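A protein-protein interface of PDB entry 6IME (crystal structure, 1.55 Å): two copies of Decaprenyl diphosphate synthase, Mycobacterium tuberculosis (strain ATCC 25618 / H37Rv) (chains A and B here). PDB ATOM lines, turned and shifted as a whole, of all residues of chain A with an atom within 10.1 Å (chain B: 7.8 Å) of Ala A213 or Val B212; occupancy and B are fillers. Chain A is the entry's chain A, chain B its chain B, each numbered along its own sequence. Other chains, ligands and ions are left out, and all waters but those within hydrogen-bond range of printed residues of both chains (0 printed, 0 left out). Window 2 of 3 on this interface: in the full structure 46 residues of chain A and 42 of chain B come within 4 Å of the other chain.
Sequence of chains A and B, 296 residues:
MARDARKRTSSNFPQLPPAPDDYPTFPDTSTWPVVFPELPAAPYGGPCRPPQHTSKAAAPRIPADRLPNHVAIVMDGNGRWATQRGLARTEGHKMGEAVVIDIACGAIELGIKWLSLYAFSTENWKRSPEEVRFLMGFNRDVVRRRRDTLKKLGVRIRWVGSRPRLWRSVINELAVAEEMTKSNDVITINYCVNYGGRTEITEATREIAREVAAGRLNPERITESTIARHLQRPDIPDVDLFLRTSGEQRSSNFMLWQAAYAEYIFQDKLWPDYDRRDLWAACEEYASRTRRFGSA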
ATOM      1  N   THR A 205       0.973  22.715  21.792  1.00  0.00           N
ATOM      2  CA  THR A 205       2.098  22.220  22.589  1.00  0.00           C
ATOM      3  C   THR A 205       3.282  23.193  22.529  1.00  0.00           C
ATOM      4  O   THR A 205       3.953  23.417  23.553  1.00  0.00           O
ATOM      5  CB  THR A 205       2.493  20.832  22.085  1.00  0.00           C
ATOM      6  OG1 THR A 205       1.416  19.932  22.339  1.00  0.00           O
ATOM      7  CG2 THR A 205       3.727  20.279  22.831  1.00  0.00           C
ATOM      8  N   ARG A 206       3.554  23.784  21.348  1.00  0.00           N
ATOM      9  CA  ARG A 206       4.608  24.799  21.228  1.00  0.00           C
ATOM     10  C   ARG A 206       4.330  25.991  22.124  1.00  0.00           C
ATOM     11  O   ARG A 206       5.235  26.522  22.783  1.00  0.00           O
ATOM     12  CB  ARG A 206       4.715  25.294  19.774  1.00  0.00           C
ATOM     13  CG  ARG A 206       5.490  24.405  18.867  1.00  0.00           C
ATOM     14  CD  ARG A 206       5.842  25.171  17.539  1.00  0.00           C
ATOM     15  NE  ARG A 206       6.206  24.180  16.555  1.00  0.00           N
ATOM     16  CZ  ARG A 206       5.437  23.863  15.522  1.00  0.00           C
ATOM     17  NH1 ARG A 206       4.296  24.523  15.323  1.00  0.00           N
ATOM     18  NH2 ARG A 206       5.807  22.908  14.688  1.00  0.00           N
ATOM     19  N   GLU A 207       3.085  26.470  22.119  1.00  0.00           N
ATOM     20  CA  GLU A 207       2.762  27.626  22.960  1.00  0.00           C
ATOM     21  C   GLU A 207       2.927  27.296  24.432  1.00  0.00           C
ATOM     22  O   GLU A 207       3.461  28.113  25.205  1.00  0.00           O
ATOM     23  CB  GLU A 207       1.337  28.099  22.677  1.00  0.00           C
ATOM     24  CG  GLU A 207       1.031  29.449  23.325  1.00  0.00           C
ATOM     25  CD  GLU A 207       1.912  30.621  22.840  1.00  0.00           C
ATOM     26  OE1 GLU A 207       2.477  30.561  21.726  1.00  0.00           O
ATOM     27  OE2 GLU A 207       2.046  31.612  23.609  1.00  0.00           O
ATOM     28  N   ILE A 208       2.476  26.105  24.840  1.00  0.00           N
ATOM     29  CA  ILE A 208       2.695  25.642  26.204  1.00  0.00           C
ATOM     30  C   ILE A 208       4.183  25.615  26.511  1.00  0.00           C
ATOM     31  O   ILE A 208       4.620  26.061  27.585  1.00  0.00           O
ATOM     32  CB  ILE A 208       2.049  24.252  26.374  1.00  0.00           C
ATOM     33  CG1 ILE A 208       0.537  24.462  26.454  1.00  0.00           C
ATOM     34  CG2 ILE A 208       2.544  23.557  27.680  1.00  0.00           C
ATOM     35  CD1 ILE A 208      -0.325  23.164  26.369  1.00  0.00           C
ATOM     36  N   ALA A 209       4.986  25.128  25.558  1.00  0.00           N
ATOM     37  CA  ALA A 209       6.440  25.060  25.755  1.00  0.00           C
ATOM     38  C   ALA A 209       7.060  26.442  25.907  1.00  0.00           C
ATOM     39  O   ALA A 209       7.983  26.619  26.710  1.00  0.00           O
ATOM     40  CB  ALA A 209       7.090  24.311  24.589  1.00  0.00           C
ATOM     41  N   ARG A 210       6.562  27.424  25.156  1.00  0.00           N
ATOM     42  CA  ARG A 210       7.055  28.802  25.292  1.00  0.00           C
ATOM     43  C   ARG A 210       6.735  29.335  26.679  1.00  0.00           C
ATOM     44  O   ARG A 210       7.549  30.027  27.300  1.00  0.00           O
ATOM     45  CB  ARG A 210       6.392  29.676  24.221  1.00  0.00           C
ATOM     46  CG  ARG A 210       6.838  29.332  22.812  1.00  0.00           C
ATOM     47  CD  ARG A 210       6.131  30.200  21.747  1.00  0.00           C
ATOM     48  NE  ARG A 210       6.431  29.689  20.405  1.00  0.00           N
ATOM     49  CZ  ARG A 210       5.522  29.246  19.544  1.00  0.00           C
ATOM     50  NH1 ARG A 210       4.218  29.296  19.844  1.00  0.00           N
ATOM     51  NH2 ARG A 210       5.908  28.781  18.366  1.00  0.00           N
ATOM     52  N   GLU A 211       5.540  29.042  27.178  1.00  0.00           N
ATOM     53  CA  GLU A 211       5.212  29.513  28.521  1.00  0.00           C
ATOM     54  C   GLU A 211       6.084  28.843  29.579  1.00  0.00           C
ATOM     55  O   GLU A 211       6.510  29.497  30.554  1.00  0.00           O
ATOM     56  CB  GLU A 211       3.733  29.272  28.813  1.00  0.00           C
ATOM     57  CG  GLU A 211       2.860  30.040  27.889  1.00  0.00           C
ATOM     58  CD  GLU A 211       1.405  29.786  28.149  1.00  0.00           C
ATOM     59  OE1 GLU A 211       1.101  28.967  29.043  1.00  0.00           O
ATOM     60  OE2 GLU A 211       0.572  30.416  27.462  1.00  0.00           O
ATOM     61  N   VAL A 212       6.387  27.552  29.393  1.00  0.00           N
ATOM     62  CA  VAL A 212       7.272  26.845  30.328  1.00  0.00           C
ATOM     63  C   VAL A 212       8.665  27.445  30.289  1.00  0.00           C
ATOM     64  O   VAL A 212       9.285  27.687  31.343  1.00  0.00           O
ATOM     65  CB  VAL A 212       7.323  25.347  29.997  1.00  0.00           C
ATOM     66  CG1 VAL A 212       8.447  24.653  30.824  1.00  0.00           C
ATOM     67  CG2 VAL A 212       5.948  24.680  30.278  1.00  0.00           C
ATOM     68  N   ALA A 213       9.197  27.652  29.082  1.00  0.00           N
ATOM     69  CA  ALA A 213      10.538  28.233  28.962  1.00  0.00           C
ATOM     70  C   ALA A 213      10.613  29.587  29.644  1.00  0.00           C
ATOM     71  O   ALA A 213      11.615  29.893  30.307  1.00  0.00           O
ATOM     72  CB  ALA A 213      10.933  28.346  27.488  1.00  0.00           C
ATOM     73  N   ALA A 214       9.543  30.385  29.556  1.00  0.00           N
ATOM     74  CA  ALA A 214       9.528  31.727  30.142  1.00  0.00           C
ATOM     75  C   ALA A 214       9.207  31.733  31.631  1.00  0.00           C
ATOM     76  O   ALA A 214       9.146  32.823  32.218  1.00  0.00           O
ATOM     77  CB  ALA A 214       8.508  32.593  29.413  1.00  0.00           C
ATOM     78  N   GLY A 215       8.964  30.575  32.241  1.00  0.00           N
ATOM     79  CA  GLY A 215       8.641  30.516  33.639  1.00  0.00           C
ATOM     80  C   GLY A 215       7.218  30.871  33.975  1.00  0.00           C
ATOM     81  O   GLY A 215       6.905  31.021  35.163  1.00  0.00           O
ATOM     82  N   ARG A 216       6.334  30.968  32.977  1.00  0.00           N
ATOM     83  CA  ARG A 216       4.934  31.313  33.206  1.00  0.00           C
ATOM     84  C   ARG A 216       4.044  30.093  33.436  1.00  0.00           C
ATOM     85  O   ARG A 216       2.879  30.263  33.820  1.00  0.00           O
ATOM     86  CB  ARG A 216       4.375  32.120  32.029  1.00  0.00           C
ATOM     87  CG  ARG A 216       5.174  33.409  31.694  1.00  0.00           C
ATOM     88  CD  ARG A 216       4.459  34.340  30.700  1.00  0.00           C
ATOM     89  NE  ARG A 216       4.247  33.748  29.373  1.00  0.00           N
ATOM     90  CZ  ARG A 216       5.068  33.901  28.334  1.00  0.00           C
ATOM     91  NH1 ARG A 216       4.790  33.316  27.175  1.00  0.00           N
ATOM     92  NH2 ARG A 216       6.169  34.641  28.447  1.00  0.00           N
ATOM     93  N   LEU A 217       4.561  28.878  33.239  1.00  0.00           N
ATOM     94  CA  LEU A 217       3.753  27.680  33.391  1.00  0.00           C
ATOM     95  C   LEU A 217       4.622  26.564  33.952  1.00  0.00           C
ATOM     96  O   LEU A 217       5.710  26.306  33.437  1.00  0.00           O
ATOM     97  CB  LEU A 217       3.142  27.296  32.039  1.00  0.00           C
ATOM     98  CG  LEU A 217       2.329  25.999  32.049  1.00  0.00           C
ATOM     99  CD1 LEU A 217       1.141  26.101  32.999  1.00  0.00           C
ATOM    100  CD2 LEU A 217       1.892  25.774  30.620  1.00  0.00           C
ATOM    101  N   ASN A 218       4.135  25.914  35.007  1.00  0.00           N
ATOM    102  CA  ASN A 218       4.796  24.749  35.586  1.00  0.00           C
ATOM    103  C   ASN A 218       4.360  23.512  34.797  1.00  0.00           C
ATOM    104  O   ASN A 218       3.158  23.281  34.657  1.00  0.00           O
ATOM    105  CB  ASN A 218       4.384  24.671  37.079  1.00  0.00           C
ATOM    106  CG  ASN A 218       4.776  23.379  37.799  1.00  0.00           C
ATOM    107  OD1 ASN A 218       5.430  22.472  37.273  1.00  0.00           O
ATOM    108  ND2 ASN A 218       4.340  23.296  39.075  1.00  0.00           N
ATOM    109  N   PRO A 219       5.296  22.717  34.255  1.00  0.00           N
ATOM    110  CA  PRO A 219       4.899  21.515  33.492  1.00  0.00           C
ATOM    111  C   PRO A 219       3.957  20.615  34.239  1.00  0.00           C
ATOM    112  O   PRO A 219       3.107  19.957  33.613  1.00  0.00           O
ATOM    113  CB  PRO A 219       6.225  20.793  33.234  1.00  0.00           C
ATOM    114  CG  PRO A 219       7.241  21.887  33.230  1.00  0.00           C
ATOM    115  CD  PRO A 219       6.758  22.905  34.255  1.00  0.00           C
ATOM    116  N   ILE A 222       0.064  20.962  33.690  1.00  0.00           N
ATOM    117  CA  ILE A 222      -0.561  20.738  32.395  1.00  0.00           C
ATOM    118  C   ILE A 222      -1.595  19.626  32.485  1.00  0.00           C
ATOM    119  O   ILE A 222      -1.288  18.494  32.894  1.00  0.00           O
ATOM    120  CB  ILE A 222       0.515  20.395  31.359  1.00  0.00           C
ATOM    121  CG1 ILE A 222       1.419  21.621  31.164  1.00  0.00           C
ATOM    122  CG2 ILE A 222      -0.103  19.927  30.037  1.00  0.00           C
ATOM    123  CD1 ILE A 222       2.722  21.279  30.402  1.00  0.00           C
ATOM    124  N   THR B 205       2.677  16.001  25.920  1.00  0.00           N
ATOM    125  CA  THR B 205       2.934  17.436  26.043  1.00  0.00           C
ATOM    126  C   THR B 205       3.611  17.745  27.371  1.00  0.00           C
ATOM    127  O   THR B 205       4.531  18.578  27.415  1.00  0.00           O
ATOM    128  CB  THR B 205       1.615  18.204  25.897  1.00  0.00           C
ATOM    129  OG1 THR B 205       1.121  18.057  24.557  1.00  0.00           O
ATOM    130  CG2 THR B 205       1.790  19.745  26.161  1.00  0.00           C
ATOM    131  N   ARG B 206       3.189  17.075  28.454  1.00  0.00           N
ATOM    132  CA  ARG B 206       3.847  17.213  29.754  1.00  0.00           C
ATOM    133  C   ARG B 206       5.311  16.808  29.675  1.00  0.00           C
ATOM    134  O   ARG B 206       6.188  17.483  30.243  1.00  0.00           O
ATOM    135  CB  ARG B 206       3.142  16.356  30.814  1.00  0.00           C
ATOM    136  CG  ARG B 206       1.913  16.926  31.428  1.00  0.00           C
ATOM    137  CD  ARG B 206       1.594  16.086  32.702  1.00  0.00           C
ATOM    138  NE  ARG B 206       0.216  16.250  33.141  1.00  0.00           N
ATOM    139  CZ  ARG B 206      -0.718  15.306  33.048  1.00  0.00           C
ATOM    140  NH1 ARG B 206      -0.410  14.109  32.566  1.00  0.00           N
ATOM    141  NH2 ARG B 206      -1.957  15.547  33.470  1.00  0.00           N
ATOM    142  N   GLU B 207       5.601  15.685  29.007  1.00  0.00           N
ATOM    143  CA  GLU B 207       6.990  15.247  28.922  1.00  0.00           C
ATOM    144  C   GLU B 207       7.819  16.255  28.139  1.00  0.00           C
ATOM    145  O   GLU B 207       8.946  16.609  28.532  1.00  0.00           O
ATOM    146  CB  GLU B 207       7.114  13.876  28.258  1.00  0.00           C
ATOM    147  CG  GLU B 207       8.520  13.280  28.466  1.00  0.00           C
ATOM    148  CD  GLU B 207       9.034  13.329  29.917  1.00  0.00           C
ATOM    149  OE1 GLU B 207       8.270  13.031  30.866  1.00  0.00           O
ATOM    150  OE2 GLU B 207      10.230  13.675  30.109  1.00  0.00           O
ATOM    151  N   ILE B 208       7.267  16.725  27.022  1.00  0.00           N
ATOM    152  CA  ILE B 208       7.919  17.755  26.230  1.00  0.00           C
ATOM    153  C   ILE B 208       8.183  18.977  27.092  1.00  0.00           C
ATOM    154  O   ILE B 208       9.287  19.550  27.066  1.00  0.00           O
ATOM    155  CB  ILE B 208       7.038  18.072  25.012  1.00  0.00           C
ATOM    156  CG1 ILE B 208       7.203  16.935  24.005  1.00  0.00           C
ATOM    157  CG2 ILE B 208       7.423  19.429  24.400  1.00  0.00           C
ATOM    158  CD1 ILE B 208       6.160  16.966  22.882  1.00  0.00           C
ATOM    159  N   ALA B 209       7.186  19.387  27.880  1.00  0.00           N
ATOM    160  CA  ALA B 209       7.374  20.562  28.731  1.00  0.00           C
ATOM    161  C   ALA B 209       8.471  20.339  29.752  1.00  0.00           C
ATOM    162  O   ALA B 209       9.215  21.285  30.077  1.00  0.00           O
ATOM    163  CB  ALA B 209       6.063  20.935  29.444  1.00  0.00           C
ATOM    164  N   ARG B 210       8.574  19.107  30.296  1.00  0.00           N
ATOM    165  CA  ARG B 210       9.658  18.836  31.249  1.00  0.00           C
ATOM    166  C   ARG B 210      11.012  18.975  30.581  1.00  0.00           C
ATOM    167  O   ARG B 210      11.952  19.546  31.173  1.00  0.00           O
ATOM    168  CB  ARG B 210       9.492  17.453  31.870  1.00  0.00           C
ATOM    169  CG  ARG B 210       8.290  17.368  32.770  1.00  0.00           C
ATOM    170  CD  ARG B 210       8.144  15.949  33.304  1.00  0.00           C
ATOM    171  NE  ARG B 210       6.888  15.792  34.037  1.00  0.00           N
ATOM    172  CZ  ARG B 210       5.923  14.952  33.682  1.00  0.00           C
ATOM    173  NH1 ARG B 210       6.066  14.161  32.620  1.00  0.00           N
ATOM    174  NH2 ARG B 210       4.807  14.902  34.401  1.00  0.00           N
ATOM    175  N   GLU B 211      11.129  18.476  29.345  1.00  0.00           N
ATOM    176  CA  GLU B 211      12.388  18.624  28.604  1.00  0.00           C
ATOM    177  C   GLU B 211      12.715  20.088  28.344  1.00  0.00           C
ATOM    178  O   GLU B 211      13.881  20.507  28.441  1.00  0.00           O
ATOM    179  CB  GLU B 211      12.314  17.846  27.296  1.00  0.00           C
ATOM    180  CG  GLU B 211      12.248  16.353  27.520  1.00  0.00           C
ATOM    181  CD  GLU B 211      12.077  15.584  26.238  1.00  0.00           C
ATOM    182  OE1 GLU B 211      12.093  16.213  25.157  1.00  0.00           O
ATOM    183  OE2 GLU B 211      11.933  14.354  26.318  1.00  0.00           O
ATOM    184  N   VAL B 212      11.699  20.892  28.019  1.00  0.00           N
ATOM    185  CA  VAL B 212      11.918  22.323  27.810  1.00  0.00           C
ATOM    186  C   VAL B 212      12.418  22.978  29.095  1.00  0.00           C
ATOM    187  O   VAL B 212      13.378  23.779  29.080  1.00  0.00           O
ATOM    188  CB  VAL B 212      10.628  22.996  27.293  1.00  0.00           C
ATOM    189  CG1 VAL B 212      10.798  24.538  27.315  1.00  0.00           C
ATOM    190  CG2 VAL B 212      10.284  22.458  25.909  1.00  0.00           C
ATOM    191  N   ALA B 213      11.720  22.716  30.209  1.00  0.00           N
ATOM    192  CA  ALA B 213      12.088  23.317  31.494  1.00  0.00           C
ATOM    193  C   ALA B 213      13.519  22.964  31.863  1.00  0.00           C
ATOM    194  O   ALA B 213      14.214  23.768  32.516  1.00  0.00           O
ATOM    195  CB  ALA B 213      11.117  22.846  32.585  1.00  0.00           C
ATOM    196  N   ALA B 214      13.976  21.780  31.466  1.00  0.00           N
ATOM    197  CA  ALA B 214      15.339  21.327  31.742  1.00  0.00           C
ATOM    198  C   ALA B 214      16.361  21.872  30.749  1.00  0.00           C
ATOM    199  O   ALA B 214      17.559  21.586  30.884  1.00  0.00           O
ATOM    200  CB  ALA B 214      15.402  19.806  31.729  1.00  0.00           C
ATOM    201  N   GLY B 215      15.932  22.641  29.760  1.00  0.00           N
ATOM    202  CA  GLY B 215      16.849  23.204  28.794  1.00  0.00           C
ATOM    203  C   GLY B 215      17.330  22.233  27.740  1.00  0.00           C
ATOM    204  O   GLY B 215      18.291  22.553  27.021  1.00  0.00           O
ATOM    205  N   ARG B 216      16.657  21.080  27.588  1.00  0.00           N
ATOM    206  CA  ARG B 216      17.030  20.029  26.647  1.00  0.00           C
ATOM    207  C   ARG B 216      16.235  20.072  25.349  1.00  0.00           C
ATOM    208  O   ARG B 216      16.530  19.298  24.425  1.00  0.00           O
ATOM    209  CB  ARG B 216      16.844  18.652  27.292  1.00  0.00           C
ATOM    210  CG  ARG B 216      17.767  18.407  28.500  1.00  0.00           C
ATOM    211  CD  ARG B 216      17.789  16.929  28.882  1.00  0.00           C
ATOM    212  NE  ARG B 216      16.481  16.441  29.312  1.00  0.00           N
ATOM    213  CZ  ARG B 216      16.099  16.340  30.585  1.00  0.00           C
ATOM    214  NH1 ARG B 216      14.882  15.891  30.884  1.00  0.00           N
ATOM    215  NH2 ARG B 216      16.935  16.683  31.560  1.00  0.00           N
ATOM    216  N   LEU B 217      15.224  20.930  25.265  1.00  0.00           N
ATOM    217  CA  LEU B 217      14.391  21.000  24.071  1.00  0.00           C
ATOM    218  C   LEU B 217      13.961  22.443  23.877  1.00  0.00           C
ATOM    219  O   LEU B 217      13.502  23.092  24.825  1.00  0.00           O
ATOM    220  CB  LEU B 217      13.167  20.083  24.200  1.00  0.00           C
ATOM    221  CG  LEU B 217      12.138  20.108  23.065  1.00  0.00           C
ATOM    222  CD1 LEU B 217      12.757  19.635  21.760  1.00  0.00           C
ATOM    223  CD2 LEU B 217      11.003  19.175  23.467  1.00  0.00           C
ATOM    224  N   ASN B 218      14.157  22.979  22.636  1.00  0.00           N
ATOM    225  CA  ASN B 218      13.721  24.330  22.360  1.00  0.00           C
ATOM    226  C   ASN B 218      12.307  24.304  21.782  1.00  0.00           C
ATOM    227  O   ASN B 218      12.028  23.493  20.881  1.00  0.00           O
ATOM    228  CB  ASN B 218      14.654  25.050  21.375  1.00  0.00           C
ATOM    229  CG  ASN B 218      14.200  26.482  21.094  1.00  0.00           C
ATOM    230  OD1 ASN B 218      13.431  26.723  20.184  1.00  0.00           O
ATOM    231  ND2 ASN B 218      14.699  27.431  21.869  1.00  0.00           N
ATOM    232  N   PRO B 219      11.413  25.168  22.271  1.00  0.00           N
ATOM    233  CA  PRO B 219      10.038  25.205  21.736  1.00  0.00           C
ATOM    234  C   PRO B 219       9.943  25.302  20.228  1.00  0.00           C
ATOM    235  O   PRO B 219       9.026  24.700  19.643  1.00  0.00           O
ATOM    236  CB  PRO B 219       9.452  26.457  22.388  1.00  0.00           C
ATOM    237  CG  PRO B 219      10.181  26.569  23.691  1.00  0.00           C
ATOM    238  CD  PRO B 219      11.596  26.072  23.425  1.00  0.00           C
ATOM    239  N   GLU B 220      10.860  26.039  19.577  1.00  0.00           N
ATOM    240  CA  GLU B 220      10.751  26.245  18.144  1.00  0.00           C
ATOM    241  C   GLU B 220      11.288  25.068  17.353  1.00  0.00           C
ATOM    242  O   GLU B 220      11.255  25.098  16.118  1.00  0.00           O
ATOM    243  CB  GLU B 220      11.488  27.525  17.714  1.00  0.00           C
ATOM    244  CG  GLU B 220      11.045  28.782  18.520  1.00  0.00           C
ATOM    245  CD  GLU B 220       9.529  28.971  18.669  1.00  0.00           C
ATOM    246  OE1 GLU B 220       8.753  28.627  17.748  1.00  0.00           O
ATOM    247  OE2 GLU B 220       9.103  29.437  19.772  1.00  0.00           O
ATOM    248  N   ILE B 222      10.015  22.000  18.200  1.00  0.00           N
ATOM    249  CA  ILE B 222       8.935  21.019  18.350  1.00  0.00           C
ATOM    250  C   ILE B 222       8.179  20.856  17.035  1.00  0.00           C
ATOM    251  O   ILE B 222       7.720  21.837  16.422  1.00  0.00           O
ATOM    252  CB  ILE B 222       7.974  21.442  19.468  1.00  0.00           C
ATOM    253  CG1 ILE B 222       8.704  21.386  20.813  1.00  0.00           C
ATOM    254  CG2 ILE B 222       6.701  20.541  19.472  1.00  0.00           C
ATOM    255  CD1 ILE B 222       7.933  22.084  21.926  1.00  0.00           C
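Ala A213 touches just one residue of chain B: Val B212 (3.8 Å). Printed residues of chain A within 4 Å of Thr B205: Thr A205 (2.9 Å). Printed residues of chain A within 4 Å of Arg B206: Pro A219 and Ile A222. Of chain A, only Val A212 (3.5 Å), Pro A219 (3.8 Å) and Ile A222 (3.5 Å) come within 4 Å of Ala B209. Val B212 touches just these residues of chain A: Ala A209 (3.6 Å) and Ala A213 (3.8 Å). No residue of chain A comes within 4 Å of Ala B214. No residue of chain A comes within 4 Å of Gly B215. Arg B216 touches none of the printed residues of chain A. No residue of chain A comes within 4 Å of Leu B217. The nearest residue of chain B that does not touch Ala A213 is Pro B219 (4.3 Å). The nearest printed residue of chain B that does not touch Thr A205 is Ile B208 (4.1 Å).
Arg A206 touches Ile B222, and with the chains exchanged Ile A222 touches Arg B206. Ala A209 touches Pro B219, and with the chains exchanged Pro A219 touches Ala B209. Ala A209 touches Ile B222, and with the chains exchanged Ile A222 touches Ala B209. Val A212 touches Ala B213, and with the chains exchanged Ala A213 touches Val B212.
Pro B219 touches Arg A206. CG1 of Val B212 touches O of Ala A209 (3.6 Å). Ile B222 touches Ala A209 (CD1 to CB, 3.6 Å). CG of Arg A210 touches CB of Pro B219, 3.9 Å away. Ala B209 touches Val A212. Val A212 touches Ala B213 (CG1 to CB, 3.7 Å). Val B212 touches Ala A213 (CG1 to CB, 3.8 Å). Pro A219 touches Arg B206 (O to CG, 3.9 Å). Pro A219 touches Ala B209. Ile A222 touches Ala B209 (CD1 to CB, 3.5 Å).
The side-chain hydroxyl of Thr B205 sits at hydrogen-bond distance from the side-chain hydroxyl of Thr A205 (2.9 Å). The guanidinium group (NE) of Arg A206 is in hydrogen-bond range of the backbone carbonyl oxygen (O) of Ile B222, 2.8 Å away. The side-chain carboxylate of Glu B220 lies within salt-bridge range of the guanidinium group of Arg A210, at 2.8 Å. The backbone carbonyl oxygen (O) of Ile A222 is in hydrogen-bond range of the guanidinium group (NE) of Arg B206 (2.7 Å).
OE1 of Glu A207 is in salt-bridge range of NH1 of Arg A210. N of Glu B220 is in hydrogen-bond range of OD1 of Asn B218, at 2.7 Å.
Hydrophobic or aromatic side chains of chain B within 4 Å of the printed part of chain A: Ala B209, Val B212, Ala B213, Pro B219 and Ile B222.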
